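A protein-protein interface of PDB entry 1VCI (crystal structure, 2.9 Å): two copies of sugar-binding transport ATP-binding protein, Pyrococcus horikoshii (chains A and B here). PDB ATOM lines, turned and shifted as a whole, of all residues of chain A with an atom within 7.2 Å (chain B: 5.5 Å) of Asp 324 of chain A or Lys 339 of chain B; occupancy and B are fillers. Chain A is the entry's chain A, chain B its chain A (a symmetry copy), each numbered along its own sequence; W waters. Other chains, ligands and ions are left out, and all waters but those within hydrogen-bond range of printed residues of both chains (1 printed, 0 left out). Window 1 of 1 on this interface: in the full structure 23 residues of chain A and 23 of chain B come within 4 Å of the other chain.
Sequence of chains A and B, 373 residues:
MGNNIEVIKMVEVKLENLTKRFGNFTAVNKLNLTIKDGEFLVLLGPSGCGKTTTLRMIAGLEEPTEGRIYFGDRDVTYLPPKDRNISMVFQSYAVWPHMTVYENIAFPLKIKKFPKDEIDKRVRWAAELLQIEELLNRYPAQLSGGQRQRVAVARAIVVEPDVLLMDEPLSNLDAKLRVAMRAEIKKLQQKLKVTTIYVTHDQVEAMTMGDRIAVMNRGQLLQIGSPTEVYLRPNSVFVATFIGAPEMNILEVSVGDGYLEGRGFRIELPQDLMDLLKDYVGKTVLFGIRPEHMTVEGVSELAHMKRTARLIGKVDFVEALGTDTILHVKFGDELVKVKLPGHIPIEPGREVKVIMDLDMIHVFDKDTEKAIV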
ATOM      1  N   VAL A 318      32.728  15.927 -19.008  1.00  0.00           N
ATOM      2  CA  VAL A 318      31.447  16.611 -19.004  1.00  0.00           C
ATOM      3  C   VAL A 318      30.267  15.656 -18.961  1.00  0.00           C
ATOM      4  O   VAL A 318      30.256  14.618 -19.623  1.00  0.00           O
ATOM      5  CB  VAL A 318      31.286  17.506 -20.242  1.00  0.00           C
ATOM      6  CG1 VAL A 318      29.957  18.242 -20.176  1.00  0.00           C
ATOM      7  CG2 VAL A 318      32.446  18.476 -20.331  1.00  0.00           C
ATOM      8  N   GLU A 319      29.276  16.023 -18.161  1.00  0.00           N
ATOM      9  CA  GLU A 319      28.064  15.245 -18.024  1.00  0.00           C
ATOM     10  C   GLU A 319      26.941  16.094 -18.601  1.00  0.00           C
ATOM     11  O   GLU A 319      26.332  16.898 -17.892  1.00  0.00           O
ATOM     12  CB  GLU A 319      27.782  14.952 -16.555  1.00  0.00           C
ATOM     13  CG  GLU A 319      28.781  14.041 -15.879  1.00  0.00           C
ATOM     14  CD  GLU A 319      28.410  13.785 -14.433  1.00  0.00           C
ATOM     15  OE1 GLU A 319      27.266  13.361 -14.180  1.00  0.00           O
ATOM     16  OE2 GLU A 319      29.256  14.007 -13.548  1.00  0.00           O
ATOM     17  N   ALA A 320      26.689  15.934 -19.894  1.00  0.00           N
ATOM     18  CA  ALA A 320      25.636  16.680 -20.564  1.00  0.00           C
ATOM     19  C   ALA A 320      24.337  15.896 -20.405  1.00  0.00           C
ATOM     20  O   ALA A 320      23.946  15.127 -21.276  1.00  0.00           O
ATOM     21  CB  ALA A 320      25.982  16.848 -22.025  1.00  0.00           C
ATOM     22  N   LEU A 321      23.669  16.097 -19.277  1.00  0.00           N
ATOM     23  CA  LEU A 321      22.435  15.384 -18.982  1.00  0.00           C
ATOM     24  C   LEU A 321      21.193  16.038 -19.575  1.00  0.00           C
ATOM     25  O   LEU A 321      20.066  15.691 -19.214  1.00  0.00           O
ATOM     26  CB  LEU A 321      22.293  15.245 -17.462  1.00  0.00           C
ATOM     27  CG  LEU A 321      23.573  14.691 -16.828  1.00  0.00           C
ATOM     28  CD1 LEU A 321      23.485  14.722 -15.314  1.00  0.00           C
ATOM     29  CD2 LEU A 321      23.806  13.276 -17.341  1.00  0.00           C
ATOM     30  N   GLY A 322      21.406  16.978 -20.491  1.00  0.00           N
ATOM     31  CA  GLY A 322      20.292  17.660 -21.123  1.00  0.00           C
ATOM     32  C   GLY A 322      19.690  18.753 -20.265  1.00  0.00           C
ATOM     33  O   GLY A 322      19.656  19.912 -20.670  1.00  0.00           O
ATOM     34  N   THR A 323      19.211  18.390 -19.079  1.00  0.00           N
ATOM     35  CA  THR A 323      18.604  19.356 -18.167  1.00  0.00           C
ATOM     36  C   THR A 323      19.636  20.024 -17.273  1.00  0.00           C
ATOM     37  O   THR A 323      19.336  20.993 -16.579  1.00  0.00           O
ATOM     38  CB  THR A 323      17.546  18.695 -17.276  1.00  0.00           C
ATOM     39  OG1 THR A 323      17.013  19.672 -16.374  1.00  0.00           O
ATOM     40  CG2 THR A 323      18.152  17.549 -16.487  1.00  0.00           C
ATOM     41  N   ASP A 324      20.849  19.486 -17.290  1.00  0.00           N
ATOM     42  CA  ASP A 324      21.956  20.012 -16.499  1.00  0.00           C
ATOM     43  C   ASP A 324      23.260  19.608 -17.158  1.00  0.00           C
ATOM     44  O   ASP A 324      23.326  18.588 -17.849  1.00  0.00           O
ATOM     45  CB  ASP A 324      21.934  19.460 -15.069  1.00  0.00           C
ATOM     46  CG  ASP A 324      20.924  20.158 -14.189  1.00  0.00           C
ATOM     47  OD1 ASP A 324      20.993  21.399 -14.074  1.00  0.00           O
ATOM     48  OD2 ASP A 324      20.065  19.468 -13.605  1.00  0.00           O
ATOM     49  N   THR A 325      24.295  20.409 -16.941  1.00  0.00           N
ATOM     50  CA  THR A 325      25.602  20.125 -17.506  1.00  0.00           C
ATOM     51  C   THR A 325      26.634  20.173 -16.397  1.00  0.00           C
ATOM     52  O   THR A 325      27.084  21.244 -16.003  1.00  0.00           O
ATOM     53  CB  THR A 325      25.956  21.139 -18.601  1.00  0.00           C
ATOM     54  OG1 THR A 325      25.144  20.891 -19.756  1.00  0.00           O
ATOM     55  CG2 THR A 325      27.422  21.032 -18.972  1.00  0.00           C
ATOM     56  N   ILE A 326      27.003  19.004 -15.894  1.00  0.00           N
ATOM     57  CA  ILE A 326      27.965  18.910 -14.806  1.00  0.00           C
ATOM     58  C   ILE A 326      29.377  18.816 -15.347  1.00  0.00           C
ATOM     59  O   ILE A 326      29.694  17.909 -16.106  1.00  0.00           O
ATOM     60  CB  ILE A 326      27.671  17.679 -13.936  1.00  0.00           C
ATOM     61  CG1 ILE A 326      26.204  17.696 -13.516  1.00  0.00           C
ATOM     62  CG2 ILE A 326      28.555  17.683 -12.706  1.00  0.00           C
ATOM     63  CD1 ILE A 326      25.750  16.438 -12.829  1.00  0.00           C
ATOM     64  N   LYS A 339      28.111  22.760 -11.600  1.00  0.00           N
ATOM     65  CA  LYS A 339      26.802  22.466 -12.160  1.00  0.00           C
ATOM     66  C   LYS A 339      26.195  23.642 -12.924  1.00  0.00           C
ATOM     67  O   LYS A 339      25.919  24.692 -12.347  1.00  0.00           O
ATOM     68  CB  LYS A 339      25.852  22.025 -11.046  1.00  0.00           C
ATOM     69  CG  LYS A 339      24.551  21.436 -11.556  1.00  0.00           C
ATOM     70  CD  LYS A 339      23.606  21.100 -10.423  1.00  0.00           C
ATOM     71  CE  LYS A 339      22.267  20.643 -10.961  1.00  0.00           C
ATOM     72  NZ  LYS A 339      21.272  20.431  -9.884  1.00  0.00           N
ATOM     73  N   LEU A 340      25.984  23.451 -14.223  1.00  0.00           N
ATOM     74  CA  LEU A 340      25.402  24.483 -15.072  1.00  0.00           C
ATOM     75  C   LEU A 340      24.041  24.018 -15.591  1.00  0.00           C
ATOM     76  O   LEU A 340      23.916  22.913 -16.118  1.00  0.00           O
ATOM     77  CB  LEU A 340      26.318  24.770 -16.260  1.00  0.00           C
ATOM     78  CG  LEU A 340      27.804  25.022 -15.999  1.00  0.00           C
ATOM     79  CD1 LEU A 340      28.498  25.326 -17.322  1.00  0.00           C
ATOM     80  CD2 LEU A 340      27.982  26.180 -15.028  1.00  0.00           C
ATOM     81  N   PRO A 341      23.003  24.856 -15.443  1.00  0.00           N
ATOM     82  CA  PRO A 341      21.648  24.520 -15.902  1.00  0.00           C
ATOM     83  C   PRO A 341      21.584  24.372 -17.413  1.00  0.00           C
ATOM     84  O   PRO A 341      22.319  25.038 -18.134  1.00  0.00           O
ATOM     85  CB  PRO A 341      20.813  25.701 -15.414  1.00  0.00           C
ATOM     86  CG  PRO A 341      21.560  26.165 -14.196  1.00  0.00           C
ATOM     87  CD  PRO A 341      22.992  26.106 -14.665  1.00  0.00           C
ATOM     88  N   GLY A 342      20.709  23.496 -17.892  1.00  0.00           N
ATOM     89  CA  GLY A 342      20.579  23.299 -19.324  1.00  0.00           C
ATOM     90  C   GLY A 342      21.605  22.356 -19.924  1.00  0.00           C
ATOM     91  O   GLY A 342      22.391  21.734 -19.210  1.00  0.00           O
ATOM     92  N   HIS A 343      21.594  22.263 -21.252  1.00  0.00           N
ATOM     93  CA  HIS A 343      22.501  21.391 -21.994  1.00  0.00           C
ATOM     94  C   HIS A 343      23.633  22.231 -22.577  1.00  0.00           C
ATOM     95  O   HIS A 343      23.454  22.916 -23.584  1.00  0.00           O
ATOM     96  CB  HIS A 343      21.722  20.693 -23.120  1.00  0.00           C
ATOM     97  CG  HIS A 343      22.424  19.511 -23.721  1.00  0.00           C
ATOM     98  ND1 HIS A 343      22.861  18.439 -22.972  1.00  0.00           N
ATOM     99  CD2 HIS A 343      22.705  19.204 -25.011  1.00  0.00           C
ATOM    100  CE1 HIS A 343      23.379  17.525 -23.773  1.00  0.00           C
ATOM    101  NE2 HIS A 343      23.296  17.964 -25.015  1.00  0.00           N
ATOM    102  N   ILE A 344      24.795  22.182 -21.934  1.00  0.00           N
ATOM    103  CA  ILE A 344      25.963  22.940 -22.384  1.00  0.00           C
ATOM    104  C   ILE A 344      27.143  21.978 -22.539  1.00  0.00           C
ATOM    105  O   ILE A 344      28.110  22.036 -21.777  1.00  0.00           O
ATOM    106  CB  ILE A 344      26.326  24.036 -21.364  1.00  0.00           C
ATOM    107  CG1 ILE A 344      25.067  24.822 -20.987  1.00  0.00           C
ATOM    108  CG2 ILE A 344      27.361  24.978 -21.957  1.00  0.00           C
ATOM    109  CD1 ILE A 344      25.276  25.835 -19.885  1.00  0.00           C
ATOM    110  N   ALA B 245      14.830  14.231 -16.389  1.00  0.00           N
ATOM    111  CA  ALA B 245      13.945  14.169 -15.232  1.00  0.00           C
ATOM    112  C   ALA B 245      14.173  15.371 -14.327  1.00  0.00           C
ATOM    113  O   ALA B 245      15.316  15.751 -14.069  1.00  0.00           O
ATOM    114  CB  ALA B 245      14.181  12.877 -14.463  1.00  0.00           C
ATOM    115  N   PRO B 246      13.086  15.992 -13.834  1.00  0.00           N
ATOM    116  CA  PRO B 246      11.671  15.660 -14.056  1.00  0.00           C
ATOM    117  C   PRO B 246      11.285  15.485 -15.525  1.00  0.00           C
ATOM    118  O   PRO B 246      11.769  16.208 -16.398  1.00  0.00           O
ATOM    119  CB  PRO B 246      10.940  16.839 -13.422  1.00  0.00           C
ATOM    120  CG  PRO B 246      11.864  17.260 -12.331  1.00  0.00           C
ATOM    121  CD  PRO B 246      13.206  17.200 -12.998  1.00  0.00           C
ATOM    122  N   PRO B 291      10.211  20.822 -17.930  1.00  0.00           N
ATOM    123  CA  PRO B 291      10.241  21.619 -16.704  1.00  0.00           C
ATOM    124  C   PRO B 291      11.419  22.579 -16.677  1.00  0.00           C
ATOM    125  O   PRO B 291      11.337  23.652 -16.090  1.00  0.00           O
ATOM    126  CB  PRO B 291      10.341  20.559 -15.620  1.00  0.00           C
ATOM    127  CG  PRO B 291       9.490  19.478 -16.175  1.00  0.00           C
ATOM    128  CD  PRO B 291       9.961  19.405 -17.611  1.00  0.00           C
ATOM    129  N   GLU B 292      12.515  22.189 -17.316  1.00  0.00           N
ATOM    130  CA  GLU B 292      13.700  23.031 -17.352  1.00  0.00           C
ATOM    131  C   GLU B 292      13.610  24.083 -18.450  1.00  0.00           C
ATOM    132  O   GLU B 292      14.467  24.959 -18.535  1.00  0.00           O
ATOM    133  CB  GLU B 292      14.969  22.182 -17.540  1.00  0.00           C
ATOM    134  CG  GLU B 292      15.055  21.411 -18.852  1.00  0.00           C
ATOM    135  CD  GLU B 292      14.509  19.999 -18.756  1.00  0.00           C
ATOM    136  OE1 GLU B 292      13.379  19.821 -18.258  1.00  0.00           O
ATOM    137  OE2 GLU B 292      15.209  19.060 -19.189  1.00  0.00           O
ATOM    138  N   MET B 294      11.008  26.083 -18.731  1.00  0.00           N
ATOM    139  CA  MET B 294       9.989  26.999 -18.235  1.00  0.00           C
ATOM    140  C   MET B 294      10.606  27.771 -17.083  1.00  0.00           C
ATOM    141  O   MET B 294      11.778  27.580 -16.760  1.00  0.00           O
ATOM    142  CB  MET B 294       8.768  26.231 -17.728  1.00  0.00           C
ATOM    143  CG  MET B 294       8.054  25.427 -18.785  1.00  0.00           C
ATOM    144  SD  MET B 294       6.795  24.353 -18.089  1.00  0.00           S
ATOM    145  CE  MET B 294       5.387  25.445 -18.100  1.00  0.00           C
ATOM    146  N   ASP B 324      18.066  22.521  -6.490  1.00  0.00           N
ATOM    147  CA  ASP B 324      17.019  22.755  -7.479  1.00  0.00           C
ATOM    148  C   ASP B 324      15.697  22.920  -6.758  1.00  0.00           C
ATOM    149  O   ASP B 324      15.507  22.386  -5.662  1.00  0.00           O
ATOM    150  CB  ASP B 324      16.904  21.583  -8.460  1.00  0.00           C
ATOM    151  CG  ASP B 324      17.971  21.608  -9.529  1.00  0.00           C
ATOM    152  OD1 ASP B 324      18.083  22.632 -10.234  1.00  0.00           O
ATOM    153  OD2 ASP B 324      18.695  20.602  -9.671  1.00  0.00           O
ATOM    154  N   THR B 325      14.784  23.658  -7.376  1.00  0.00           N
ATOM    155  CA  THR B 325      13.472  23.881  -6.795  1.00  0.00           C
ATOM    156  C   THR B 325      12.417  23.538  -7.827  1.00  0.00           C
ATOM    157  O   THR B 325      12.115  24.337  -8.709  1.00  0.00           O
ATOM    158  CB  THR B 325      13.314  25.339  -6.344  1.00  0.00           C
ATOM    159  OG1 THR B 325      14.126  25.566  -5.183  1.00  0.00           O
ATOM    160  CG2 THR B 325      11.864  25.644  -6.025  1.00  0.00           C
ATOM    161  N   ILE B 326      11.859  22.341  -7.713  1.00  0.00           N
ATOM    162  CA  ILE B 326      10.852  21.875  -8.656  1.00  0.00           C
ATOM    163  C   ILE B 326       9.464  22.266  -8.192  1.00  0.00           C
ATOM    164  O   ILE B 326       9.046  21.899  -7.101  1.00  0.00           O
ATOM    165  CB  ILE B 326      10.927  20.348  -8.807  1.00  0.00           C
ATOM    166  CG1 ILE B 326      12.363  19.941  -9.126  1.00  0.00           C
ATOM    167  CG2 ILE B 326      10.007  19.887  -9.918  1.00  0.00           C
ATOM    168  CD1 ILE B 326      12.599  18.457  -9.098  1.00  0.00           C
ATOM    169  N   LEU B 327       8.750  23.008  -9.028  1.00  0.00           N
ATOM    170  CA  LEU B 327       7.406  23.451  -8.683  1.00  0.00           C
ATOM    171  C   LEU B 327       6.314  22.688  -9.418  1.00  0.00           C
ATOM    172  O   LEU B 327       6.460  22.343 -10.591  1.00  0.00           O
ATOM    173  CB  LEU B 327       7.247  24.938  -8.984  1.00  0.00           C
ATOM    174  CG  LEU B 327       8.283  25.887  -8.381  1.00  0.00           C
ATOM    175  CD1 LEU B 327       7.928  27.314  -8.773  1.00  0.00           C
ATOM    176  CD2 LEU B 327       8.321  25.728  -6.866  1.00  0.00           C
ATOM    177  N   LYS B 337       5.249  20.576 -13.983  1.00  0.00           N
ATOM    178  CA  LYS B 337       6.416  20.792 -13.143  1.00  0.00           C
ATOM    179  C   LYS B 337       7.355  21.804 -13.772  1.00  0.00           C
ATOM    180  O   LYS B 337       7.671  21.716 -14.954  1.00  0.00           O
ATOM    181  CB  LYS B 337       7.185  19.485 -12.931  1.00  0.00           C
ATOM    182  CG  LYS B 337       6.452  18.427 -12.138  1.00  0.00           C
ATOM    183  CD  LYS B 337       7.304  17.188 -12.027  1.00  0.00           C
ATOM    184  CE  LYS B 337       6.568  16.067 -11.333  1.00  0.00           C
ATOM    185  NZ  LYS B 337       7.341  14.796 -11.392  1.00  0.00           N
ATOM    186  N   VAL B 338       7.795  22.768 -12.976  1.00  0.00           N
ATOM    187  CA  VAL B 338       8.728  23.778 -13.454  1.00  0.00           C
ATOM    188  C   VAL B 338      10.016  23.602 -12.652  1.00  0.00           C
ATOM    189  O   VAL B 338       9.976  23.405 -11.436  1.00  0.00           O
ATOM    190  CB  VAL B 338       8.175  25.211 -13.256  1.00  0.00           C
ATOM    191  CG1 VAL B 338       9.222  26.232 -13.656  1.00  0.00           C
ATOM    192  CG2 VAL B 338       6.940  25.403 -14.100  1.00  0.00           C
ATOM    193  N   LYS B 339      11.156  23.660 -13.330  1.00  0.00           N
ATOM    194  CA  LYS B 339      12.426  23.484 -12.647  1.00  0.00           C
ATOM    195  C   LYS B 339      13.230  24.778 -12.527  1.00  0.00           C
ATOM    196  O   LYS B 339      13.637  25.362 -13.529  1.00  0.00           O
ATOM    197  CB  LYS B 339      13.257  22.422 -13.370  1.00  0.00           C
ATOM    198  CG  LYS B 339      14.475  21.970 -12.588  1.00  0.00           C
ATOM    199  CD  LYS B 339      15.315  20.990 -13.379  1.00  0.00           C
ATOM    200  CE  LYS B 339      16.592  20.659 -12.636  1.00  0.00           C
ATOM    201  NZ  LYS B 339      17.502  19.806 -13.435  1.00  0.00           N
ATOM    202  N   LEU B 340      13.461  25.212 -11.291  1.00  0.00           N
ATOM    203  CA  LEU B 340      14.222  26.427 -11.028  1.00  0.00           C
ATOM    204  C   LEU B 340      15.517  26.076 -10.296  1.00  0.00           C
ATOM    205  O   LEU B 340      15.497  25.361  -9.295  1.00  0.00           O
ATOM    206  CB  LEU B 340      13.405  27.386 -10.164  1.00  0.00           C
ATOM    207  CG  LEU B 340      11.964  27.698 -10.572  1.00  0.00           C
ATOM    208  CD1 LEU B 340      11.375  28.704  -9.591  1.00  0.00           C
ATOM    209  CD2 LEU B 340      11.922  28.250 -11.989  1.00  0.00           C
ATOM    210  N   PRO B 341      16.662  26.573 -10.792  1.00  0.00           N
ATOM    211  CA  PRO B 341      17.969  26.305 -10.175  1.00  0.00           C
ATOM    212  C   PRO B 341      18.068  26.901  -8.781  1.00  0.00           C
ATOM    213  O   PRO B 341      17.469  27.934  -8.503  1.00  0.00           O
ATOM    214  CB  PRO B 341      18.951  26.962 -11.143  1.00  0.00           C
ATOM    215  CG  PRO B 341      18.234  26.882 -12.461  1.00  0.00           C
ATOM    216  CD  PRO B 341      16.828  27.271 -12.077  1.00  0.00           C
HETATM  217  O   HOH W   1      14.100  18.659 -16.177  1.00  0.00           O
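The backbone carbonyl oxygen (O) of Gly 342 of chain A sits close to the backbone NH (N) of Asp 324 of chain A (3.3 Å). The backbone carbonyl oxygen (O) of Pro 291 of chain B lies within hydrogen-bond range of the backbone NH (N) of Lys 339 of chain B. The backbone carbonyl oxygen of Thr 323 of chain A lies within hydrogen-bond range of the backbone NH of Gly 342 of chain A (3.1 Å).
The side-chain amino group of Lys 339 of chain B sits at hydrogen-bond distance from the side-chain hydroxyl of Thr 323 of chain A (3.0 Å). The side-chain carboxylate (OD2) of Asp 324 of chain A lies within salt-bridge range of the side-chain amino group (NZ) of Lys 339 of chain B (2.6 Å). The side-chain hydroxyl (OG1) of Thr 323 of chain A sits close to the side-chain carboxylate (OE2) of Glu 292 of chain B (3.4 Å). NZ of Lys 339 of chain A lies within salt-bridge range of OD2 of Asp 324 of chain B, at 2.6 Å.
Of the 15 printed residues of chain A, 4 touch a printed residue of chain B. Hydrophobic or aromatic side chains of chain A within 4 Å of the printed part of chain B: Pro 341. Of the 14 printed residues of chain B, 4 touch a printed residue of chain A. Along chain B the printed residues that touch a printed residue of chain A span positions 292 to 341. Among the printed residues, 5 pairs touch across the chains. Among the printed residues, Asp or Glu carboxylates within 4 Å of a Lys or Arg side-chain nitrogen of the other chain: Asp 324 of chain A with Lys 339 of chain B (2.6 Å) and Lys 339 of chain A with Asp 324 of chain B (2.6 Å).
Among the printed residues, pairs that only touch across the chains: Pro 341 of chain A with Pro 341 of chain B (3.8 Å).
Water W1 lies within hydrogen-bond range of OE1 of Glu 292 of chain B, OG1 of Thr 323 of chain A and O of Pro 246 of chain B.
Of chain B, only Lys 339 comes within 4 Å of Asp 324 of chain A. Lys 339 of chain B touches just these residues of chain A: Thr 323 (3.0 Å) and Asp 324 (2.6 Å). Of the printed residues of chain A, Pro 341 of chain B touches Pro 341. Of the printed residues of chain B, Pro 341 of chain A touches Pro 341. Of the printed residues of chain A, Glu 292 of chain B touches Thr 323. Leu 340 of chain A touches none of the printed residues of chain B. The nearest residue of chain B that does not touch Asp 324 of chain A is Asp 324 of chain B (4.3 Å). The nearest residue of chain A that does not touch Lys 339 of chain B is Lys 339 of chain A (5.2 Å).
Asp 324 of chain A touches Lys 339 of chain B, and with the chains exchanged Lys 339 of chain A touches Asp 324 of chain B. Pro 341 of chain B touches its own counterpart, Pro 341 of chain A. 6 positions are printed for both chains. Of the 5 pairs that touch across the chains among the printed residues, 3 have their exchanged pair printed and touching as well.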
